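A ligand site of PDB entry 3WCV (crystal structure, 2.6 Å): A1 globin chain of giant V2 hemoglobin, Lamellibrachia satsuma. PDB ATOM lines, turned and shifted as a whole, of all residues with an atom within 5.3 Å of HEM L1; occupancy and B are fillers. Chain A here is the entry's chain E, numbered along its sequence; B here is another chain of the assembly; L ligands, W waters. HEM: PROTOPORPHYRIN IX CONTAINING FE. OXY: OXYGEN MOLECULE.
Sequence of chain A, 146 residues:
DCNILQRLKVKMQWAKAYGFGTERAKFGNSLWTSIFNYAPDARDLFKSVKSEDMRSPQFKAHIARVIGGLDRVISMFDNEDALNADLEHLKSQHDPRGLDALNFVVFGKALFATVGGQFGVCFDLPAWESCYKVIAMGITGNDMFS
An oxygen (O1A) of HEM L1 lies within hydrogen-bond range of a ring nitrogen (NE2) of His 94 of chain B, at 3.2 Å. NE2 of Gln 98 of chain B lies within hydrogen-bond range of O2A of HEM L1. FE of HEM L1 is bound by NE2 of His 94 of chain A (2.1 Å). An oxygen (O2A) of HEM L1 lies close to the side-chain amide nitrogen (NE2) of Gln 93 (3.4 Å). NE2 of Gln 93 is in hydrogen-bond range of O2A of HEM L3 (3.3 Å). The side-chain hydroxyl (OG) of Ser 48 lies within hydrogen-bond range of an oxygen (O1D) of HEM L1, at 2.5 Å. NE2 of Gln 98 of chain B lies close to O2A of HEM L3, at 3.5 Å. An oxygen (O1D) of HEM L1 is in salt-bridge range of the guanidinium group (NH2) of Arg 97 (3.5 Å). An oxygen (O2) of OXY L2 is in hydrogen-bond range of a ring nitrogen (NE2) of His 62 (2.9 Å).
An oxygen (O1) of OXY L2 binds an iron atom (FE) of HEM L1 (1.8 Å).
The side-chain hydroxyl (OH) of Tyr 132 is in hydrogen-bond range of the backbone carbonyl oxygen (O) of Phe 104. ND1 of His 94 of chain A lies within hydrogen-bond range of O of Leu 90 (2.8 Å).
Merely in contact with HEM L1: Phe 46 (3.4 Å), Phe 107 (3.4 Å), Phe 104 (3.4 Å), Val 49 (3.4 Å), Arg 65 (3.5 Å), Leu 45 (3.5 Å), Ile 139 (3.7 Å), Tyr 132 (3.7 Å), Asn 103 (3.8 Å), His 62 (3.8 Å), Leu 99 (3.8 Å), Leu 90 (3.9 Å) and Ile 135 (3.9 Å). Hydrophobic or aromatic side chains within 4 Å of HEM L1: Leu 45, Phe 46, Val 49, His 62, Leu 90, His 94 of chain A, Leu 99, Phe 104, Phe 107, Tyr 132, Ile 135, Ile 139 and His 94 of chain B. The nearest printed residue that does not touch HEM L1 is Val 66 (4.1 Å).
Water W1 lies within hydrogen-bond range of the guanidinium group of Arg 65 (2.8 Å), an oxygen (O2D) of HEM L1 (2.9 Å) and a ring nitrogen (ND1) of His 62 (3.1 Å).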
ATOM      1  N   TRP A  32      27.522 -36.441   7.489  1.00  0.00           N
ATOM      2  CA  TRP A  32      26.512 -37.246   6.830  1.00  0.00           C
ATOM      3  C   TRP A  32      26.635 -38.762   7.051  1.00  0.00           C
ATOM      4  O   TRP A  32      25.648 -39.490   6.929  1.00  0.00           O
ATOM      5  CB  TRP A  32      26.428 -36.895   5.334  1.00  0.00           C
ATOM      6  CG  TRP A  32      25.698 -35.601   5.150  1.00  0.00           C
ATOM      7  CD1 TRP A  32      26.253 -34.360   5.004  1.00  0.00           C
ATOM      8  CD2 TRP A  32      24.286 -35.408   5.139  1.00  0.00           C
ATOM      9  NE1 TRP A  32      25.267 -33.395   4.902  1.00  0.00           N
ATOM     10  CE2 TRP A  32      24.051 -34.020   4.984  1.00  0.00           C
ATOM     11  CE3 TRP A  32      23.188 -36.269   5.246  1.00  0.00           C
ATOM     12  CZ2 TRP A  32      22.759 -33.476   4.928  1.00  0.00           C
ATOM     13  CZ3 TRP A  32      21.906 -35.734   5.199  1.00  0.00           C
ATOM     14  CH2 TRP A  32      21.701 -34.348   5.039  1.00  0.00           C
ATOM     15  N   ALA A  42      16.716 -42.347   6.854  1.00  0.00           N
ATOM     16  CA  ALA A  42      16.737 -40.986   6.343  1.00  0.00           C
ATOM     17  C   ALA A  42      17.437 -40.941   4.981  1.00  0.00           C
ATOM     18  O   ALA A  42      17.219 -40.035   4.185  1.00  0.00           O
ATOM     19  CB  ALA A  42      17.442 -40.083   7.328  1.00  0.00           C
ATOM     20  N   LEU A  45      15.509 -40.386   1.658  1.00  0.00           N
ATOM     21  CA  LEU A  45      14.981 -39.063   1.374  1.00  0.00           C
ATOM     22  C   LEU A  45      15.886 -38.287   0.430  1.00  0.00           C
ATOM     23  O   LEU A  45      15.535 -37.215  -0.068  1.00  0.00           O
ATOM     24  CB  LEU A  45      14.828 -38.300   2.687  1.00  0.00           C
ATOM     25  CG  LEU A  45      14.029 -39.061   3.748  1.00  0.00           C
ATOM     26  CD1 LEU A  45      14.036 -38.270   5.037  1.00  0.00           C
ATOM     27  CD2 LEU A  45      12.608 -39.263   3.255  1.00  0.00           C
ATOM     28  N   PHE A  46      17.044 -38.854   0.152  1.00  0.00           N
ATOM     29  CA  PHE A  46      18.015 -38.184  -0.690  1.00  0.00           C
ATOM     30  C   PHE A  46      18.316 -38.807  -2.035  1.00  0.00           C
ATOM     31  O   PHE A  46      19.404 -38.571  -2.593  1.00  0.00           O
ATOM     32  CB  PHE A  46      19.309 -37.989   0.083  1.00  0.00           C
ATOM     33  CG  PHE A  46      19.130 -37.162   1.313  1.00  0.00           C
ATOM     34  CD1 PHE A  46      19.239 -35.776   1.244  1.00  0.00           C
ATOM     35  CD2 PHE A  46      18.806 -37.747   2.518  1.00  0.00           C
ATOM     36  CE1 PHE A  46      19.013 -34.987   2.362  1.00  0.00           C
ATOM     37  CE2 PHE A  46      18.580 -36.976   3.648  1.00  0.00           C
ATOM     38  CZ  PHE A  46      18.678 -35.591   3.570  1.00  0.00           C
ATOM     39  N   SER A  48      17.266 -37.975  -4.728  1.00  0.00           N
ATOM     40  CA  SER A  48      17.468 -36.866  -5.667  1.00  0.00           C
ATOM     41  C   SER A  48      18.933 -36.417  -5.757  1.00  0.00           C
ATOM     42  O   SER A  48      19.331 -35.775  -6.724  1.00  0.00           O
ATOM     43  CB  SER A  48      16.614 -35.671  -5.259  1.00  0.00           C
ATOM     44  OG  SER A  48      16.830 -35.367  -3.886  1.00  0.00           O
ATOM     45  N   VAL A  49      19.735 -36.745  -4.753  1.00  0.00           N
ATOM     46  CA  VAL A  49      21.144 -36.358  -4.770  1.00  0.00           C
ATOM     47  C   VAL A  49      22.030 -37.576  -4.756  1.00  0.00           C
ATOM     48  O   VAL A  49      23.148 -37.526  -4.250  1.00  0.00           O
ATOM     49  CB  VAL A  49      21.530 -35.486  -3.568  1.00  0.00           C
ATOM     50  CG1 VAL A  49      21.030 -34.066  -3.762  1.00  0.00           C
ATOM     51  CG2 VAL A  49      20.952 -36.090  -2.287  1.00  0.00           C
ATOM     52  N   HIS A  62      26.066 -32.227  -2.609  1.00  0.00           N
ATOM     53  CA  HIS A  62      24.993 -31.975  -1.648  1.00  0.00           C
ATOM     54  C   HIS A  62      25.621 -31.696  -0.277  1.00  0.00           C
ATOM     55  O   HIS A  62      25.210 -30.773   0.429  1.00  0.00           O
ATOM     56  CB  HIS A  62      24.031 -33.177  -1.552  1.00  0.00           C
ATOM     57  CG  HIS A  62      23.070 -33.086  -0.410  1.00  0.00           C
ATOM     58  ND1 HIS A  62      22.037 -32.177  -0.379  1.00  0.00           N
ATOM     59  CD2 HIS A  62      23.032 -33.740   0.774  1.00  0.00           C
ATOM     60  CE1 HIS A  62      21.397 -32.286   0.768  1.00  0.00           C
ATOM     61  NE2 HIS A  62      21.977 -33.220   1.487  1.00  0.00           N
ATOM     62  N   ARG A  65      26.822 -28.235  -0.148  1.00  0.00           N
ATOM     63  CA  ARG A  65      25.733 -27.256  -0.045  1.00  0.00           C
ATOM     64  C   ARG A  65      25.173 -27.143   1.376  1.00  0.00           C
ATOM     65  O   ARG A  65      24.877 -26.036   1.850  1.00  0.00           O
ATOM     66  CB  ARG A  65      24.594 -27.609  -1.018  1.00  0.00           C
ATOM     67  CG  ARG A  65      24.801 -27.119  -2.453  1.00  0.00           C
ATOM     68  CD  ARG A  65      23.520 -27.290  -3.291  1.00  0.00           C
ATOM     69  NE  ARG A  65      23.192 -28.689  -3.505  1.00  0.00           N
ATOM     70  CZ  ARG A  65      23.724 -29.451  -4.464  1.00  0.00           C
ATOM     71  NH1 ARG A  65      24.592 -28.927  -5.321  1.00  0.00           N
ATOM     72  NH2 ARG A  65      23.390 -30.737  -4.545  1.00  0.00           N
ATOM     73  N   VAL A  66      25.068 -28.281   2.062  1.00  0.00           N
ATOM     74  CA  VAL A  66      24.562 -28.308   3.427  1.00  0.00           C
ATOM     75  C   VAL A  66      25.532 -27.670   4.430  1.00  0.00           C
ATOM     76  O   VAL A  66      25.109 -26.865   5.259  1.00  0.00           O
ATOM     77  CB  VAL A  66      24.275 -29.757   3.890  1.00  0.00           C
ATOM     78  CG1 VAL A  66      23.938 -29.782   5.384  1.00  0.00           C
ATOM     79  CG2 VAL A  66      23.134 -30.371   3.040  1.00  0.00           C
ATOM     80  N   GLY A  69      25.488 -24.230   4.067  1.00  0.00           N
ATOM     81  CA  GLY A  69      24.300 -23.606   4.628  1.00  0.00           C
ATOM     82  C   GLY A  69      24.513 -23.402   6.122  1.00  0.00           C
ATOM     83  O   GLY A  69      24.166 -22.372   6.709  1.00  0.00           O
ATOM     84  N   LEU A  70      25.117 -24.407   6.743  1.00  0.00           N
ATOM     85  CA  LEU A  70      25.414 -24.325   8.164  1.00  0.00           C
ATOM     86  C   LEU A  70      26.364 -23.154   8.386  1.00  0.00           C
ATOM     87  O   LEU A  70      26.142 -22.325   9.278  1.00  0.00           O
ATOM     88  CB  LEU A  70      26.058 -25.638   8.634  1.00  0.00           C
ATOM     89  CG  LEU A  70      25.120 -26.831   8.838  1.00  0.00           C
ATOM     90  CD1 LEU A  70      25.885 -28.108   8.893  1.00  0.00           C
ATOM     91  CD2 LEU A  70      24.342 -26.659  10.101  1.00  0.00           C
ATOM     92  N   ARG A  72      27.093 -20.303   6.482  1.00  0.00           N
ATOM     93  CA  ARG A  72      26.527 -18.968   6.294  1.00  0.00           C
ATOM     94  C   ARG A  72      25.482 -18.639   7.357  1.00  0.00           C
ATOM     95  O   ARG A  72      25.373 -17.479   7.760  1.00  0.00           O
ATOM     96  CB  ARG A  72      25.885 -18.855   4.912  1.00  0.00           C
ATOM     97  CG  ARG A  72      24.636 -19.660   4.761  1.00  0.00           C
ATOM     98  CD  ARG A  72      24.178 -19.705   3.317  1.00  0.00           C
ATOM     99  NE  ARG A  72      22.727 -19.815   3.255  1.00  0.00           N
ATOM    100  CZ  ARG A  72      22.062 -20.653   2.462  1.00  0.00           C
ATOM    101  NH1 ARG A  72      22.720 -21.451   1.642  1.00  0.00           N
ATOM    102  NH2 ARG A  72      20.738 -20.684   2.478  1.00  0.00           N
ATOM    103  N   LEU A  90      15.695 -21.135   3.519  1.00  0.00           N
ATOM    104  CA  LEU A  90      15.977 -22.556   3.671  1.00  0.00           C
ATOM    105  C   LEU A  90      14.705 -23.346   3.885  1.00  0.00           C
ATOM    106  O   LEU A  90      14.563 -24.469   3.390  1.00  0.00           O
ATOM    107  CB  LEU A  90      16.946 -22.779   4.826  1.00  0.00           C
ATOM    108  CG  LEU A  90      18.394 -22.368   4.539  1.00  0.00           C
ATOM    109  CD1 LEU A  90      19.178 -22.307   5.827  1.00  0.00           C
ATOM    110  CD2 LEU A  90      19.008 -23.340   3.547  1.00  0.00           C
ATOM    111  N   GLN A  93      12.937 -24.085   0.709  1.00  0.00           N
ATOM    112  CA  GLN A  93      13.541 -25.175  -0.049  1.00  0.00           C
ATOM    113  C   GLN A  93      13.235 -26.562   0.543  1.00  0.00           C
ATOM    114  O   GLN A  93      13.233 -27.554  -0.194  1.00  0.00           O
ATOM    115  CB  GLN A  93      15.059 -24.992  -0.134  1.00  0.00           C
ATOM    116  CG  GLN A  93      15.473 -23.714  -0.852  1.00  0.00           C
ATOM    117  CD  GLN A  93      16.964 -23.545  -0.902  1.00  0.00           C
ATOM    118  OE1 GLN A  93      17.626 -23.611   0.129  1.00  0.00           O
ATOM    119  NE2 GLN A  93      17.508 -23.313  -2.087  1.00  0.00           N
ATOM    120  N   HIS A  94      12.972 -26.618   1.847  1.00  0.00           N
ATOM    121  CA  HIS A  94      12.680 -27.900   2.489  1.00  0.00           C
ATOM    122  C   HIS A  94      11.194 -28.273   2.616  1.00  0.00           C
ATOM    123  O   HIS A  94      10.867 -29.464   2.698  1.00  0.00           O
ATOM    124  CB  HIS A  94      13.338 -27.953   3.884  1.00  0.00           C
ATOM    125  CG  HIS A  94      14.829 -28.066   3.837  1.00  0.00           C
ATOM    126  ND1 HIS A  94      15.659 -27.003   3.568  1.00  0.00           N
ATOM    127  CD2 HIS A  94      15.656 -29.134   4.019  1.00  0.00           C
ATOM    128  CE1 HIS A  94      16.918 -27.397   3.596  1.00  0.00           C
ATOM    129  NE2 HIS A  94      16.942 -28.691   3.872  1.00  0.00           N
ATOM    130  N   ARG A  97       9.122 -30.734   0.323  1.00  0.00           N
ATOM    131  CA  ARG A  97       9.650 -32.081   0.456  1.00  0.00           C
ATOM    132  C   ARG A  97       9.003 -32.853   1.599  1.00  0.00           C
ATOM    133  O   ARG A  97       9.335 -34.018   1.844  1.00  0.00           O
ATOM    134  CB  ARG A  97      11.163 -32.013   0.635  1.00  0.00           C
ATOM    135  CG  ARG A  97      11.805 -30.954  -0.237  1.00  0.00           C
ATOM    136  CD  ARG A  97      13.262 -31.242  -0.457  1.00  0.00           C
ATOM    137  NE  ARG A  97      13.500 -31.799  -1.778  1.00  0.00           N
ATOM    138  CZ  ARG A  97      14.036 -31.109  -2.798  1.00  0.00           C
ATOM    139  NH1 ARG A  97      14.381 -29.845  -2.615  1.00  0.00           N
ATOM    140  NH2 ARG A  97      14.208 -31.700  -3.976  1.00  0.00           N
ATOM    141  N   LEU A  99       9.113 -33.131   5.018  1.00  0.00           N
ATOM    142  CA  LEU A  99      10.044 -33.875   5.847  1.00  0.00           C
ATOM    143  C   LEU A  99       9.564 -33.957   7.284  1.00  0.00           C
ATOM    144  O   LEU A  99       9.039 -32.988   7.860  1.00  0.00           O
ATOM    145  CB  LEU A  99      11.414 -33.184   5.821  1.00  0.00           C
ATOM    146  CG  LEU A  99      12.074 -32.985   4.461  1.00  0.00           C
ATOM    147  CD1 LEU A  99      13.211 -31.967   4.570  1.00  0.00           C
ATOM    148  CD2 LEU A  99      12.571 -34.329   3.951  1.00  0.00           C
ATOM    149  N   ASN A 103      13.579 -35.876  11.892  1.00  0.00           N
ATOM    150  CA  ASN A 103      14.867 -36.034  11.218  1.00  0.00           C
ATOM    151  C   ASN A 103      15.803 -34.890  11.586  1.00  0.00           C
ATOM    152  O   ASN A 103      17.017 -35.091  11.715  1.00  0.00           O
ATOM    153  CB  ASN A 103      14.702 -36.063   9.694  1.00  0.00           C
ATOM    154  CG  ASN A 103      14.269 -37.412   9.186  1.00  0.00           C
ATOM    155  OD1 ASN A 103      13.396 -37.499   8.327  1.00  0.00           O
ATOM    156  ND2 ASN A 103      14.867 -38.466   9.711  1.00  0.00           N
ATOM    157  N   PHE A 104      15.251 -33.695  11.752  1.00  0.00           N
ATOM    158  CA  PHE A 104      16.074 -32.565  12.105  1.00  0.00           C
ATOM    159  C   PHE A 104      16.673 -32.706  13.485  1.00  0.00           C
ATOM    160  O   PHE A 104      17.667 -32.062  13.795  1.00  0.00           O
ATOM    161  CB  PHE A 104      15.252 -31.269  11.994  1.00  0.00           C
ATOM    162  CG  PHE A 104      15.109 -30.775  10.586  1.00  0.00           C
ATOM    163  CD1 PHE A 104      15.928 -29.752  10.098  1.00  0.00           C
ATOM    164  CD2 PHE A 104      14.189 -31.354   9.713  1.00  0.00           C
ATOM    165  CE1 PHE A 104      15.830 -29.324   8.769  1.00  0.00           C
ATOM    166  CE2 PHE A 104      14.092 -30.935   8.395  1.00  0.00           C
ATOM    167  CZ  PHE A 104      14.902 -29.920   7.920  1.00  0.00           C
ATOM    168  N   PHE A 107      19.690 -34.905  12.843  1.00  0.00           N
ATOM    169  CA  PHE A 107      20.707 -34.079  12.194  1.00  0.00           C
ATOM    170  C   PHE A 107      21.530 -33.308  13.235  1.00  0.00           C
ATOM    171  O   PHE A 107      22.767 -33.229  13.145  1.00  0.00           O
ATOM    172  CB  PHE A 107      20.046 -33.103  11.218  1.00  0.00           C
ATOM    173  CG  PHE A 107      20.999 -32.244  10.443  1.00  0.00           C
ATOM    174  CD1 PHE A 107      21.727 -31.224  11.071  1.00  0.00           C
ATOM    175  CD2 PHE A 107      21.145 -32.409   9.061  1.00  0.00           C
ATOM    176  CE1 PHE A 107      22.570 -30.397  10.324  1.00  0.00           C
ATOM    177  CE2 PHE A 107      21.980 -31.580   8.324  1.00  0.00           C
ATOM    178  CZ  PHE A 107      22.685 -30.579   8.947  1.00  0.00           C
ATOM    179  N   TYR A 132      21.183 -24.643  18.014  1.00  0.00           N
ATOM    180  CA  TYR A 132      20.771 -25.436  16.879  1.00  0.00           C
ATOM    181  C   TYR A 132      19.256 -25.396  16.783  1.00  0.00           C
ATOM    182  O   TYR A 132      18.686 -25.472  15.681  1.00  0.00           O
ATOM    183  CB  TYR A 132      21.228 -26.882  16.990  1.00  0.00           C
ATOM    184  CG  TYR A 132      20.654 -27.743  15.893  1.00  0.00           C
ATOM    185  CD1 TYR A 132      19.573 -28.583  16.127  1.00  0.00           C
ATOM    186  CD2 TYR A 132      21.184 -27.680  14.613  1.00  0.00           C
ATOM    187  CE1 TYR A 132      19.034 -29.359  15.099  1.00  0.00           C
ATOM    188  CE2 TYR A 132      20.654 -28.447  13.573  1.00  0.00           C
ATOM    189  CZ  TYR A 132      19.577 -29.285  13.836  1.00  0.00           C
ATOM    190  OH  TYR A 132      19.050 -30.070  12.828  1.00  0.00           O
ATOM    191  N   ILE A 135      18.062 -22.769  14.587  1.00  0.00           N
ATOM    192  CA  ILE A 135      18.121 -23.123  13.171  1.00  0.00           C
ATOM    193  C   ILE A 135      16.974 -24.047  12.773  1.00  0.00           C
ATOM    194  O   ILE A 135      16.227 -23.767  11.826  1.00  0.00           O
ATOM    195  CB  ILE A 135      19.476 -23.768  12.823  1.00  0.00           C
ATOM    196  CG1 ILE A 135      20.617 -22.781  13.146  1.00  0.00           C
ATOM    197  CG2 ILE A 135      19.493 -24.147  11.334  1.00  0.00           C
ATOM    198  CD1 ILE A 135      22.037 -23.346  12.944  1.00  0.00           C
ATOM    199  N   ALA A 136      16.825 -25.150  13.492  1.00  0.00           N
ATOM    200  CA  ALA A 136      15.780 -26.111  13.194  1.00  0.00           C
ATOM    201  C   ALA A 136      14.404 -25.454  13.211  1.00  0.00           C
ATOM    202  O   ALA A 136      13.568 -25.715  12.341  1.00  0.00           O
ATOM    203  CB  ALA A 136      15.836 -27.259  14.204  1.00  0.00           C
ATOM    204  N   ILE A 139      13.945 -23.453  10.149  1.00  0.00           N
ATOM    205  CA  ILE A 139      13.795 -24.212   8.906  1.00  0.00           C
ATOM    206  C   ILE A 139      12.521 -25.040   8.810  1.00  0.00           C
ATOM    207  O   ILE A 139      11.899 -25.099   7.764  1.00  0.00           O
ATOM    208  CB  ILE A 139      15.036 -25.130   8.687  1.00  0.00           C
ATOM    209  CG1 ILE A 139      16.290 -24.266   8.610  1.00  0.00           C
ATOM    210  CG2 ILE A 139      14.864 -25.991   7.415  1.00  0.00           C
ATOM    211  CD1 ILE A 139      17.574 -25.031   8.332  1.00  0.00           C
ATOM    212  N   HIS B  94      24.019 -27.549 -10.533  1.00  0.00           N
ATOM    213  CA  HIS B  94      22.950 -27.199  -9.600  1.00  0.00           C
ATOM    214  C   HIS B  94      22.770 -25.685  -9.551  1.00  0.00           C
ATOM    215  O   HIS B  94      21.651 -25.176  -9.657  1.00  0.00           O
ATOM    216  CB  HIS B  94      23.299 -27.737  -8.215  1.00  0.00           C
ATOM    217  CG  HIS B  94      22.193 -27.590  -7.220  1.00  0.00           C
ATOM    218  ND1 HIS B  94      21.842 -26.373  -6.678  1.00  0.00           N
ATOM    219  CD2 HIS B  94      21.347 -28.498  -6.688  1.00  0.00           C
ATOM    220  CE1 HIS B  94      20.834 -26.530  -5.853  1.00  0.00           C
ATOM    221  NE2 HIS B  94      20.503 -27.816  -5.833  1.00  0.00           N
ATOM    222  N   GLN B  98      19.542 -23.098 -10.634  1.00  0.00           N
ATOM    223  CA  GLN B  98      18.944 -22.070  -9.790  1.00  0.00           C
ATOM    224  C   GLN B  98      18.831 -20.708 -10.486  1.00  0.00           C
ATOM    225  O   GLN B  98      17.996 -19.881 -10.121  1.00  0.00           O
ATOM    226  CB  GLN B  98      19.736 -21.927  -8.480  1.00  0.00           C
ATOM    227  CG  GLN B  98      19.760 -23.220  -7.647  1.00  0.00           C
ATOM    228  CD  GLN B  98      20.467 -23.069  -6.305  1.00  0.00           C
ATOM    229  OE1 GLN B  98      21.608 -22.618  -6.241  1.00  0.00           O
ATOM    230  NE2 GLN B  98      19.787 -23.454  -5.232  1.00  0.00           N
HETATM  231  CHA HEM L   1      18.680 -29.609   0.561  1.00  0.00           C
HETATM  232  CHB HEM L   1      20.532 -27.205   4.183  1.00  0.00           C
HETATM  233  CHC HEM L   1      18.701 -30.393   7.304  1.00  0.00           C
HETATM  234  CHD HEM L   1      16.799 -32.781   3.595  1.00  0.00           C
HETATM  235  C1A HEM L   1      19.363 -28.669   1.272  1.00  0.00           C
HETATM  236  C2A HEM L   1      20.048 -27.618   0.669  1.00  0.00           C
HETATM  237  C3A HEM L   1      20.581 -26.922   1.694  1.00  0.00           C
HETATM  238  C4A HEM L   1      20.208 -27.561   2.940  1.00  0.00           C
HETATM  239  CMA HEM L   1      21.438 -25.643   1.605  1.00  0.00           C
HETATM  240  CAA HEM L   1      20.175 -27.327  -0.800  1.00  0.00           C
HETATM  241  CBA HEM L   1      19.160 -26.347  -1.304  1.00  0.00           C
HETATM  242  CGA HEM L   1      19.285 -26.058  -2.792  1.00  0.00           C
HETATM  243  O1A HEM L   1      18.551 -26.683  -3.614  1.00  0.00           O
HETATM  244  O2A HEM L   1      20.105 -25.273  -3.138  1.00  0.00           O
HETATM  245  C1B HEM L   1      20.187 -27.848   5.406  1.00  0.00           C
HETATM  246  C2B HEM L   1      20.599 -27.370   6.719  1.00  0.00           C
HETATM  247  C3B HEM L   1      20.050 -28.350   7.633  1.00  0.00           C
HETATM  248  C4B HEM L   1      19.365 -29.289   6.820  1.00  0.00           C
HETATM  249  CMB HEM L   1      21.421 -26.163   7.025  1.00  0.00           C
HETATM  250  CAB HEM L   1      20.238 -28.270   9.079  1.00  0.00           C
HETATM  251  CBB HEM L   1      19.382 -27.797   9.952  1.00  0.00           C
HETATM  252  C1C HEM L   1      18.013 -31.327   6.542  1.00  0.00           C
HETATM  253  C2C HEM L   1      17.330 -32.470   7.133  1.00  0.00           C
HETATM  254  C3C HEM L   1      16.752 -33.195   6.085  1.00  0.00           C
HETATM  255  C4C HEM L   1      17.147 -32.405   4.854  1.00  0.00           C
HETATM  256  CMC HEM L   1      17.263 -32.802   8.627  1.00  0.00           C
HETATM  257  CAC HEM L   1      16.034 -34.342   6.165  1.00  0.00           C
HETATM  258  CBC HEM L   1      16.223 -35.609   6.296  1.00  0.00           C
HETATM  259  C1D HEM L   1      17.133 -32.113   2.432  1.00  0.00           C
HETATM  260  C2D HEM L   1      16.742 -32.569   1.034  1.00  0.00           C
HETATM  261  C3D HEM L   1      17.289 -31.641   0.206  1.00  0.00           C
HETATM  262  C4D HEM L   1      17.999 -30.671   1.043  1.00  0.00           C
HETATM  263  CMD HEM L   1      15.899 -33.804   0.733  1.00  0.00           C
HETATM  264  CAD HEM L   1      17.214 -31.583  -1.297  1.00  0.00           C
HETATM  265  CBD HEM L   1      18.342 -32.275  -1.976  1.00  0.00           C
HETATM  266  CGD HEM L   1      18.226 -32.150  -3.439  1.00  0.00           C
HETATM  267  O1D HEM L   1      17.518 -32.964  -4.107  1.00  0.00           O
HETATM  268  O2D HEM L   1      18.828 -31.230  -3.990  1.00  0.00           O
HETATM  269  NA  HEM L   1      19.449 -28.667   2.668  1.00  0.00           N
HETATM  270  NB  HEM L   1      19.454 -28.968   5.435  1.00  0.00           N
HETATM  271  NC  HEM L   1      17.878 -31.334   5.163  1.00  0.00           N
HETATM  272  ND  HEM L   1      17.871 -30.996   2.363  1.00  0.00           N
HETATM  273 FE   HEM L   1      18.643 -29.985   3.907  1.00  0.00          FE
HETATM  274  O1  OXY L   2      20.011 -31.120   3.931  1.00  0.00           O
HETATM  275  O2  OXY L   2      20.080 -32.306   3.546  1.00  0.00           O
HETATM  276  CHA HEM L   3      20.553 -16.508  -6.662  1.00  0.00           C
HETATM  277  CHB HEM L   3      25.191 -17.581  -6.702  1.00  0.00           C
HETATM  278  CHC HEM L   3      25.952 -14.532 -10.377  1.00  0.00           C
HETATM  279  CHD HEM L   3      21.269 -13.507 -10.348  1.00  0.00           C
HETATM  280  C1A HEM L   3      21.777 -17.084  -6.331  1.00  0.00           C
HETATM  281  C2A HEM L   3      21.956 -18.014  -5.275  1.00  0.00           C
HETATM  282  C3A HEM L   3      23.256 -18.314  -5.291  1.00  0.00           C
HETATM  283  C4A HEM L   3      23.911 -17.575  -6.360  1.00  0.00           C
HETATM  284  CMA HEM L   3      23.994 -19.287  -4.346  1.00  0.00           C
HETATM  285  CAA HEM L   3      20.915 -18.550  -4.333  1.00  0.00           C
HETATM  286  CBA HEM L   3      20.276 -19.816  -4.841  1.00  0.00           C
HETATM  287  CGA HEM L   3      19.208 -20.404  -3.932  1.00  0.00           C
HETATM  288  O1A HEM L   3      18.005 -20.354  -4.282  1.00  0.00           O
HETATM  289  O2A HEM L   3      19.567 -20.894  -2.896  1.00  0.00           O
HETATM  290  C1B HEM L   3      25.851 -16.848  -7.721  1.00  0.00           C
HETATM  291  C2B HEM L   3      27.267 -16.936  -7.982  1.00  0.00           C
HETATM  292  C3B HEM L   3      27.486 -16.013  -9.080  1.00  0.00           C
HETATM  293  C4B HEM L   3      26.205 -15.471  -9.371  1.00  0.00           C
HETATM  294  CMB HEM L   3      28.266 -17.777  -7.285  1.00  0.00           C
HETATM  295  CAB HEM L   3      28.793 -15.772  -9.668  1.00  0.00           C
HETATM  296  CBB HEM L   3      29.219 -16.322 -10.782  1.00  0.00           C
HETATM  297  C1C HEM L   3      24.719 -13.984 -10.684  1.00  0.00           C
HETATM  298  C2C HEM L   3      24.541 -13.005 -11.755  1.00  0.00           C
HETATM  299  C3C HEM L   3      23.167 -12.674 -11.782  1.00  0.00           C
HETATM  300  C4C HEM L   3      22.570 -13.523 -10.671  1.00  0.00           C
HETATM  301  CMC HEM L   3      25.648 -12.459 -12.656  1.00  0.00           C
HETATM  302  CAC HEM L   3      22.528 -11.797 -12.611  1.00  0.00           C
HETATM  303  CBC HEM L   3      22.514 -10.542 -12.866  1.00  0.00           C
HETATM  304  C1D HEM L   3      20.657 -14.234  -9.345  1.00  0.00           C
HETATM  305  C2D HEM L   3      19.176 -14.148  -9.035  1.00  0.00           C
HETATM  306  C3D HEM L   3      18.987 -15.006  -7.976  1.00  0.00           C
HETATM  307  C4D HEM L   3      20.318 -15.590  -7.669  1.00  0.00           C
HETATM  308  CMD HEM L   3      18.185 -13.253  -9.788  1.00  0.00           C
HETATM  309  CAD HEM L   3      17.682 -15.287  -7.274  1.00  0.00           C
HETATM  310  CBD HEM L   3      17.504 -14.411  -6.058  1.00  0.00           C
HETATM  311  CGD HEM L   3      16.236 -14.651  -5.323  1.00  0.00           C
HETATM  312  O1D HEM L   3      16.000 -15.760  -4.734  1.00  0.00           O
HETATM  313  O2D HEM L   3      15.397 -13.732  -5.279  1.00  0.00           O
HETATM  314  NA  HEM L   3      22.975 -16.803  -6.999  1.00  0.00           N
HETATM  315  NB  HEM L   3      25.183 -16.007  -8.522  1.00  0.00           N
HETATM  316  NC  HEM L   3      23.504 -14.268 -10.064  1.00  0.00           N
HETATM  317  ND  HEM L   3      21.276 -15.092  -8.526  1.00  0.00           N
HETATM  318 FE   HEM L   3      23.222 -15.551  -8.543  1.00  0.00          FE
HETATM  319  O   HOH W   1      21.037 -30.165  -2.459  1.00  0.00           O
